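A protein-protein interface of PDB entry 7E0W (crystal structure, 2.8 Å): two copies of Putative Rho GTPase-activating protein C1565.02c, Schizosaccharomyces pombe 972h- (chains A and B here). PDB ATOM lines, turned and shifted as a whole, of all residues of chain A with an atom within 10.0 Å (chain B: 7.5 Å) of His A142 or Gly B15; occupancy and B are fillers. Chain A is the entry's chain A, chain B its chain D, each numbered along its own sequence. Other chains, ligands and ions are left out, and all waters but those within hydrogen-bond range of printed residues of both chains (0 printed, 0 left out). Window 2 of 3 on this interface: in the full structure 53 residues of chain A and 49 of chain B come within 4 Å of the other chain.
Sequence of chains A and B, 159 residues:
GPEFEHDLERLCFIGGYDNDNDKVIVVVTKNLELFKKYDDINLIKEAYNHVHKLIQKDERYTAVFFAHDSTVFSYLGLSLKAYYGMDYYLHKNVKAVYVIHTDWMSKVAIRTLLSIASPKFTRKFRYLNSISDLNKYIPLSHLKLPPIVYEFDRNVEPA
Among the printed residues, pairs that only touch across the chains: Leu A143 with Gly B15 (3.1 Å), His A142 with Tyr B17 (3.2 Å), His A142 with Gly B16 (3.4 Å), Leu A143 with Val B24 (3.6 Å), Leu A143 with Gly B16 (3.7 Å) and His A142 with Gly B15 (3.8 Å).
No position is printed for both chains.
No residue of chain B comes within 4 Å of Ser A141. His A142 touches just these residues of chain B: Gly B15, Gly B16 and Tyr B17. Of the printed residues of chain B, Leu A143 touches Gly B15 (3.1 Å), Gly B16 (3.7 Å) and Val B24 (3.6 Å). Gly B15 touches just these residues of chain A: His A142, Leu A143 and Lys A144. Asn B19 touches none of the printed residues of chain A. Printed residues of chain A within 4 Å of Val B24: Leu A143. The nearest residue of chain A that does not touch Gly B15 is Leu A145 (5.3 Å). The nearest printed residue of chain A that does not touch Val B24 is Ile A138 (4.5 Å).
The backbone NH (N) of Lys A144 is in hydrogen-bond range of the backbone carbonyl oxygen (O) of Gly B15.
Of the 13 printed residues of chain A, 3 touch a printed residue of chain B. Printed residues of chain B that touch a printed residue of chain A: Gly B15, Gly B16, Tyr B17 and Val B24. Hydrophobic or aromatic side chains of chain B within 4 Å of the printed part of chain A: Val B24. Among the printed residues, 7 pairs touch across the chains. Among the printed residues, no Asp or Glu carboxylate lies within 4 Å of a Lys or Arg side-chain nitrogen of the other chain.
The side-chain hydroxyl of Ser A141 sits at hydrogen-bond distance from a ring nitrogen (ND1) of His A142. The backbone carbonyl oxygen (O) of Gly B16 lies within hydrogen-bond range of the backbone NH (N) of Val B24, at 3.2 Å.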
ATOM      1  N   LEU A 134       4.581  23.276  31.309  1.00  0.00           N
ATOM      2  CA  LEU A 134       4.658  23.345  29.856  1.00  0.00           C
ATOM      3  C   LEU A 134       3.840  24.505  29.291  1.00  0.00           C
ATOM      4  O   LEU A 134       4.211  25.050  28.246  1.00  0.00           O
ATOM      5  CB  LEU A 134       4.197  22.000  29.267  1.00  0.00           C
ATOM      6  CG  LEU A 134       4.577  21.465  27.876  1.00  0.00           C
ATOM      7  CD1 LEU A 134       4.106  20.007  27.694  1.00  0.00           C
ATOM      8  CD2 LEU A 134       4.027  22.336  26.773  1.00  0.00           C
ATOM      9  N   ASN A 135       2.801  24.948  30.014  1.00  0.00           N
ATOM     10  CA  ASN A 135       1.716  25.733  29.420  1.00  0.00           C
ATOM     11  C   ASN A 135       2.215  26.934  28.631  1.00  0.00           C
ATOM     12  O   ASN A 135       1.667  27.259  27.572  1.00  0.00           O
ATOM     13  CB  ASN A 135       0.737  26.185  30.508  1.00  0.00           C
ATOM     14  CG  ASN A 135      -0.718  26.115  30.054  1.00  0.00           C
ATOM     15  OD1 ASN A 135      -1.005  26.095  28.857  1.00  0.00           O
ATOM     16  ND2 ASN A 135      -1.641  26.072  31.012  1.00  0.00           N
ATOM     17  N   TYR A 137       4.943  27.577  26.817  1.00  0.00           N
ATOM     18  CA  TYR A 137       5.549  27.398  25.499  1.00  0.00           C
ATOM     19  C   TYR A 137       4.570  26.730  24.519  1.00  0.00           C
ATOM     20  O   TYR A 137       4.363  27.281  23.415  1.00  0.00           O
ATOM     21  CB  TYR A 137       6.837  26.581  25.630  1.00  0.00           C
ATOM     22  CG  TYR A 137       7.673  26.992  26.824  1.00  0.00           C
ATOM     23  CD1 TYR A 137       7.477  26.407  28.069  1.00  0.00           C
ATOM     24  CD2 TYR A 137       8.640  27.983  26.711  1.00  0.00           C
ATOM     25  CE1 TYR A 137       8.228  26.788  29.164  1.00  0.00           C
ATOM     26  CE2 TYR A 137       9.397  28.369  27.800  1.00  0.00           C
ATOM     27  CZ  TYR A 137       9.187  27.769  29.023  1.00  0.00           C
ATOM     28  OH  TYR A 137       9.940  28.152  30.109  1.00  0.00           O
ATOM     29  N   ILE A 138       4.002  25.631  24.869  1.00  0.00           N
ATOM     30  CA  ILE A 138       3.010  24.923  24.041  1.00  0.00           C
ATOM     31  C   ILE A 138       1.702  24.855  24.821  1.00  0.00           C
ATOM     32  O   ILE A 138       1.724  24.446  25.990  1.00  0.00           O
ATOM     33  CB  ILE A 138       3.464  23.523  23.616  1.00  0.00           C
ATOM     34  CG1 ILE A 138       4.279  23.576  22.318  1.00  0.00           C
ATOM     35  CG2 ILE A 138       2.277  22.573  23.476  1.00  0.00           C
ATOM     36  CD1 ILE A 138       5.663  24.162  22.488  1.00  0.00           C
ATOM     37  N   PRO A 139       0.575  25.251  24.250  1.00  0.00           N
ATOM     38  CA  PRO A 139      -0.701  25.130  24.972  1.00  0.00           C
ATOM     39  C   PRO A 139      -1.173  23.681  25.004  1.00  0.00           C
ATOM     40  O   PRO A 139      -1.191  22.994  23.980  1.00  0.00           O
ATOM     41  CB  PRO A 139      -1.652  26.022  24.167  1.00  0.00           C
ATOM     42  CG  PRO A 139      -1.081  26.028  22.790  1.00  0.00           C
ATOM     43  CD  PRO A 139       0.414  25.928  22.948  1.00  0.00           C
ATOM     44  N   LEU A 140      -1.561  23.225  26.197  1.00  0.00           N
ATOM     45  CA  LEU A 140      -1.936  21.829  26.402  1.00  0.00           C
ATOM     46  C   LEU A 140      -3.345  21.521  25.923  1.00  0.00           C
ATOM     47  O   LEU A 140      -3.661  20.348  25.690  1.00  0.00           O
ATOM     48  CB  LEU A 140      -1.818  21.437  27.880  1.00  0.00           C
ATOM     49  CG  LEU A 140      -0.451  21.449  28.574  1.00  0.00           C
ATOM     50  CD1 LEU A 140       0.112  22.843  28.682  1.00  0.00           C
ATOM     51  CD2 LEU A 140      -0.531  20.809  29.953  1.00  0.00           C
ATOM     52  N   SER A 141      -4.198  22.538  25.787  1.00  0.00           N
ATOM     53  CA  SER A 141      -5.519  22.322  25.210  1.00  0.00           C
ATOM     54  C   SER A 141      -5.422  21.748  23.803  1.00  0.00           C
ATOM     55  O   SER A 141      -6.325  21.029  23.361  1.00  0.00           O
ATOM     56  CB  SER A 141      -6.305  23.633  25.205  1.00  0.00           C
ATOM     57  OG  SER A 141      -5.558  24.671  24.592  1.00  0.00           O
ATOM     58  N   HIS A 142      -4.329  22.041  23.095  1.00  0.00           N
ATOM     59  CA  HIS A 142      -4.123  21.555  21.737  1.00  0.00           C
ATOM     60  C   HIS A 142      -3.762  20.076  21.674  1.00  0.00           C
ATOM     61  O   HIS A 142      -3.669  19.532  20.568  1.00  0.00           O
ATOM     62  CB  HIS A 142      -3.011  22.357  21.056  1.00  0.00           C
ATOM     63  CG  HIS A 142      -3.394  23.759  20.699  1.00  0.00           C
ATOM     64  ND1 HIS A 142      -4.003  24.617  21.590  1.00  0.00           N
ATOM     65  CD2 HIS A 142      -3.236  24.458  19.551  1.00  0.00           C
ATOM     66  CE1 HIS A 142      -4.212  25.782  21.002  1.00  0.00           C
ATOM     67  NE2 HIS A 142      -3.756  25.711  19.764  1.00  0.00           N
ATOM     68  N   LEU A 143      -3.558  19.413  22.812  1.00  0.00           N
ATOM     69  CA  LEU A 143      -2.885  18.121  22.836  1.00  0.00           C
ATOM     70  C   LEU A 143      -3.723  17.066  23.546  1.00  0.00           C
ATOM     71  O   LEU A 143      -4.445  17.356  24.502  1.00  0.00           O
ATOM     72  CB  LEU A 143      -1.522  18.219  23.537  1.00  0.00           C
ATOM     73  CG  LEU A 143      -0.715  19.505  23.356  1.00  0.00           C
ATOM     74  CD1 LEU A 143       0.350  19.607  24.431  1.00  0.00           C
ATOM     75  CD2 LEU A 143      -0.091  19.567  21.975  1.00  0.00           C
ATOM     76  N   LYS A 144      -3.599  15.829  23.067  1.00  0.00           N
ATOM     77  CA  LYS A 144      -4.099  14.650  23.763  1.00  0.00           C
ATOM     78  C   LYS A 144      -2.937  13.987  24.492  1.00  0.00           C
ATOM     79  O   LYS A 144      -1.912  13.668  23.876  1.00  0.00           O
ATOM     80  CB  LYS A 144      -4.745  13.661  22.789  1.00  0.00           C
ATOM     81  CG  LYS A 144      -5.376  14.287  21.550  1.00  0.00           C
ATOM     82  CD  LYS A 144      -5.259  13.346  20.354  1.00  0.00           C
ATOM     83  CE  LYS A 144      -5.765  13.983  19.067  1.00  0.00           C
ATOM     84  NZ  LYS A 144      -5.278  13.241  17.866  1.00  0.00           N
ATOM     85  N   LEU A 145      -3.099  13.771  25.795  1.00  0.00           N
ATOM     86  CA  LEU A 145      -2.015  13.338  26.662  1.00  0.00           C
ATOM     87  C   LEU A 145      -2.378  12.037  27.374  1.00  0.00           C
ATOM     88  O   LEU A 145      -3.554  11.780  27.640  1.00  0.00           O
ATOM     89  CB  LEU A 145      -1.686  14.430  27.694  1.00  0.00           C
ATOM     90  CG  LEU A 145      -1.432  15.824  27.117  1.00  0.00           C
ATOM     91  CD1 LEU A 145      -0.910  16.769  28.192  1.00  0.00           C
ATOM     92  CD2 LEU A 145      -0.467  15.748  25.934  1.00  0.00           C
ATOM     93  N   PRO A 146      -1.380  11.217  27.704  1.00  0.00           N
ATOM     94  CA  PRO A 146      -1.657   9.844  28.159  1.00  0.00           C
ATOM     95  C   PRO A 146      -2.138   9.816  29.597  1.00  0.00           C
ATOM     96  O   PRO A 146      -2.037  10.824  30.315  1.00  0.00           O
ATOM     97  CB  PRO A 146      -0.295   9.142  28.004  1.00  0.00           C
ATOM     98  CG  PRO A 146       0.727  10.229  27.841  1.00  0.00           C
ATOM     99  CD  PRO A 146       0.048  11.558  27.820  1.00  0.00           C
ATOM    100  N   TYR A 150      -2.269  11.962  34.527  1.00  0.00           N
ATOM    101  CA  TYR A 150      -3.595  12.286  35.035  1.00  0.00           C
ATOM    102  C   TYR A 150      -3.862  11.554  36.347  1.00  0.00           C
ATOM    103  O   TYR A 150      -3.021  10.811  36.862  1.00  0.00           O
ATOM    104  CB  TYR A 150      -4.664  11.933  34.000  1.00  0.00           C
ATOM    105  CG  TYR A 150      -4.756  12.903  32.850  1.00  0.00           C
ATOM    106  CD1 TYR A 150      -4.244  14.189  32.956  1.00  0.00           C
ATOM    107  CD2 TYR A 150      -5.351  12.530  31.653  1.00  0.00           C
ATOM    108  CE1 TYR A 150      -4.325  15.077  31.903  1.00  0.00           C
ATOM    109  CE2 TYR A 150      -5.436  13.410  30.595  1.00  0.00           C
ATOM    110  CZ  TYR A 150      -4.922  14.682  30.725  1.00  0.00           C
ATOM    111  OH  TYR A 150      -5.007  15.562  29.671  1.00  0.00           O
ATOM    112  N   CYS B  12       4.613   6.871  21.492  1.00  0.00           N
ATOM    113  CA  CYS B  12       4.964   7.984  20.612  1.00  0.00           C
ATOM    114  C   CYS B  12       3.711   8.381  19.835  1.00  0.00           C
ATOM    115  O   CYS B  12       3.326   7.689  18.887  1.00  0.00           O
ATOM    116  CB  CYS B  12       6.103   7.593  19.680  1.00  0.00           C
ATOM    117  SG  CYS B  12       7.047   8.967  18.985  1.00  0.00           S
ATOM    118  N   PHE B  13       3.082   9.484  20.239  1.00  0.00           N
ATOM    119  CA  PHE B  13       1.971  10.064  19.499  1.00  0.00           C
ATOM    120  C   PHE B  13       2.386  11.388  18.879  1.00  0.00           C
ATOM    121  O   PHE B  13       3.466  11.925  19.142  1.00  0.00           O
ATOM    122  CB  PHE B  13       0.738  10.313  20.383  1.00  0.00           C
ATOM    123  CG  PHE B  13       0.614   9.389  21.553  1.00  0.00           C
ATOM    124  CD1 PHE B  13       0.584   9.881  22.844  1.00  0.00           C
ATOM    125  CD2 PHE B  13       0.511   8.034  21.371  1.00  0.00           C
ATOM    126  CE1 PHE B  13       0.476   9.041  23.928  1.00  0.00           C
ATOM    127  CE2 PHE B  13       0.401   7.196  22.458  1.00  0.00           C
ATOM    128  CZ  PHE B  13       0.379   7.700  23.738  1.00  0.00           C
ATOM    129  N   ILE B  14       1.498  11.905  18.043  1.00  0.00           N
ATOM    130  CA  ILE B  14       1.449  13.328  17.734  1.00  0.00           C
ATOM    131  C   ILE B  14       0.323  13.862  18.611  1.00  0.00           C
ATOM    132  O   ILE B  14      -0.843  13.892  18.215  1.00  0.00           O
ATOM    133  CB  ILE B  14       1.212  13.594  16.247  1.00  0.00           C
ATOM    134  CG1 ILE B  14       2.079  12.679  15.378  1.00  0.00           C
ATOM    135  CG2 ILE B  14       1.465  15.060  15.919  1.00  0.00           C
ATOM    136  CD1 ILE B  14       1.356  11.445  14.877  1.00  0.00           C
ATOM    137  N   GLY B  15       0.679  14.268  19.832  1.00  0.00           N
ATOM    138  CA  GLY B  15      -0.329  14.701  20.785  1.00  0.00           C
ATOM    139  C   GLY B  15      -1.161  15.861  20.283  1.00  0.00           C
ATOM    140  O   GLY B  15      -2.348  15.967  20.604  1.00  0.00           O
ATOM    141  N   GLY B  16      -0.564  16.729  19.475  1.00  0.00           N
ATOM    142  CA  GLY B  16      -1.273  17.858  18.915  1.00  0.00           C
ATOM    143  C   GLY B  16      -0.401  18.696  18.007  1.00  0.00           C
ATOM    144  O   GLY B  16       0.564  18.195  17.421  1.00  0.00           O
ATOM    145  N   TYR B  17      -0.738  19.976  17.880  1.00  0.00           N
ATOM    146  CA  TYR B  17      -0.015  20.894  17.015  1.00  0.00           C
ATOM    147  C   TYR B  17       0.141  22.228  17.727  1.00  0.00           C
ATOM    148  O   TYR B  17      -0.766  22.667  18.441  1.00  0.00           O
ATOM    149  CB  TYR B  17      -0.742  21.097  15.677  1.00  0.00           C
ATOM    150  CG  TYR B  17      -0.680  19.912  14.735  1.00  0.00           C
ATOM    151  CD1 TYR B  17      -1.457  18.781  14.951  1.00  0.00           C
ATOM    152  CD2 TYR B  17       0.151  19.931  13.623  1.00  0.00           C
ATOM    153  CE1 TYR B  17      -1.403  17.700  14.090  1.00  0.00           C
ATOM    154  CE2 TYR B  17       0.210  18.856  12.756  1.00  0.00           C
ATOM    155  CZ  TYR B  17      -0.568  17.743  12.996  1.00  0.00           C
ATOM    156  OH  TYR B  17      -0.511  16.671  12.135  1.00  0.00           O
ATOM    157  N   ASP B  18       1.293  22.865  17.535  1.00  0.00           N
ATOM    158  CA  ASP B  18       1.516  24.187  18.098  1.00  0.00           C
ATOM    159  C   ASP B  18       0.639  25.219  17.387  1.00  0.00           C
ATOM    160  O   ASP B  18      -0.015  24.935  16.381  1.00  0.00           O
ATOM    161  CB  ASP B  18       2.993  24.574  17.995  1.00  0.00           C
ATOM    162  CG  ASP B  18       3.554  24.403  16.591  1.00  0.00           C
ATOM    163  OD1 ASP B  18       2.794  24.532  15.609  1.00  0.00           O
ATOM    164  OD2 ASP B  18       4.765  24.134  16.468  1.00  0.00           O
ATOM    165  N   ASN B  19       0.635  26.441  17.924  1.00  0.00           N
ATOM    166  CA  ASN B  19      -0.120  27.512  17.286  1.00  0.00           C
ATOM    167  C   ASN B  19       0.512  27.951  15.973  1.00  0.00           C
ATOM    168  O   ASN B  19      -0.154  28.611  15.168  1.00  0.00           O
ATOM    169  CB  ASN B  19      -0.258  28.707  18.227  1.00  0.00           C
ATOM    170  CG  ASN B  19      -1.308  29.697  17.756  1.00  0.00           C
ATOM    171  OD1 ASN B  19      -0.991  30.694  17.109  1.00  0.00           O
ATOM    172  ND2 ASN B  19      -2.567  29.417  18.072  1.00  0.00           N
ATOM    173  N   ASP B  20       1.776  27.603  15.738  1.00  0.00           N
ATOM    174  CA  ASP B  20       2.366  27.745  14.417  1.00  0.00           C
ATOM    175  C   ASP B  20       1.993  26.592  13.497  1.00  0.00           C
ATOM    176  O   ASP B  20       2.507  26.514  12.375  1.00  0.00           O
ATOM    177  CB  ASP B  20       3.890  27.869  14.529  1.00  0.00           C
ATOM    178  CG  ASP B  20       4.324  29.230  15.042  1.00  0.00           C
ATOM    179  OD1 ASP B  20       3.542  30.195  14.909  1.00  0.00           O
ATOM    180  OD2 ASP B  20       5.446  29.335  15.583  1.00  0.00           O
ATOM    181  N   ASN B  21       1.113  25.701  13.963  1.00  0.00           N
ATOM    182  CA  ASN B  21       0.530  24.634  13.145  1.00  0.00           C
ATOM    183  C   ASN B  21       1.590  23.667  12.632  1.00  0.00           C
ATOM    184  O   ASN B  21       1.522  23.179  11.504  1.00  0.00           O
ATOM    185  CB  ASN B  21      -0.294  25.211  11.995  1.00  0.00           C
ATOM    186  CG  ASN B  21      -1.413  26.107  12.479  1.00  0.00           C
ATOM    187  OD1 ASN B  21      -1.464  27.290  12.154  1.00  0.00           O
ATOM    188  ND2 ASN B  21      -2.314  25.544  13.281  1.00  0.00           N
ATOM    189  N   LYS B  23       3.942  20.115  14.132  1.00  0.00           N
ATOM    190  CA  LYS B  23       3.648  19.000  15.018  1.00  0.00           C
ATOM    191  C   LYS B  23       4.314  19.153  16.383  1.00  0.00           C
ATOM    192  O   LYS B  23       5.260  19.924  16.572  1.00  0.00           O
ATOM    193  CB  LYS B  23       4.100  17.683  14.390  1.00  0.00           C
ATOM    194  CG  LYS B  23       3.188  17.167  13.303  1.00  0.00           C
ATOM    195  CD  LYS B  23       3.649  15.812  12.811  1.00  0.00           C
ATOM    196  CE  LYS B  23       2.818  15.349  11.633  1.00  0.00           C
ATOM    197  NZ  LYS B  23       3.422  14.157  10.984  1.00  0.00           N
ATOM    198  N   VAL B  24       3.773  18.408  17.347  1.00  0.00           N
ATOM    199  CA  VAL B  24       4.447  18.063  18.588  1.00  0.00           C
ATOM    200  C   VAL B  24       4.477  16.543  18.663  1.00  0.00           C
ATOM    201  O   VAL B  24       3.521  15.874  18.252  1.00  0.00           O
ATOM    202  CB  VAL B  24       3.761  18.675  19.833  1.00  0.00           C
ATOM    203  CG1 VAL B  24       3.380  20.132  19.589  1.00  0.00           C
ATOM    204  CG2 VAL B  24       2.535  17.870  20.251  1.00  0.00           C
ATOM    205  N   ILE B  25       5.586  15.990  19.139  1.00  0.00           N
ATOM    206  CA  ILE B  25       5.750  14.546  19.234  1.00  0.00           C
ATOM    207  C   ILE B  25       5.953  14.210  20.698  1.00  0.00           C
ATOM    208  O   ILE B  25       6.962  14.598  21.302  1.00  0.00           O
ATOM    209  CB  ILE B  25       6.908  14.027  18.374  1.00  0.00           C
ATOM    210  CG1 ILE B  25       6.699  14.441  16.921  1.00  0.00           C
ATOM    211  CG2 ILE B  25       7.008  12.511  18.478  1.00  0.00           C
ATOM    212  CD1 ILE B  25       5.522  13.750  16.259  1.00  0.00           C
ATOM    213  N   VAL B  26       5.006  13.521  21.264  1.00  0.00           N
ATOM    214  CA  VAL B  26       5.078  13.117  22.655  1.00  0.00           C
ATOM    215  C   VAL B  26       5.710  11.736  22.710  1.00  0.00           C
ATOM    216  O   VAL B  26       5.491  10.894  21.830  1.00  0.00           O
ATOM    217  CB  VAL B  26       3.678  13.146  23.292  1.00  0.00           C
ATOM    218  CG1 VAL B  26       2.960  11.874  23.032  1.00  0.00           C
ATOM    219  CG2 VAL B  26       3.784  13.389  24.757  1.00  0.00           C
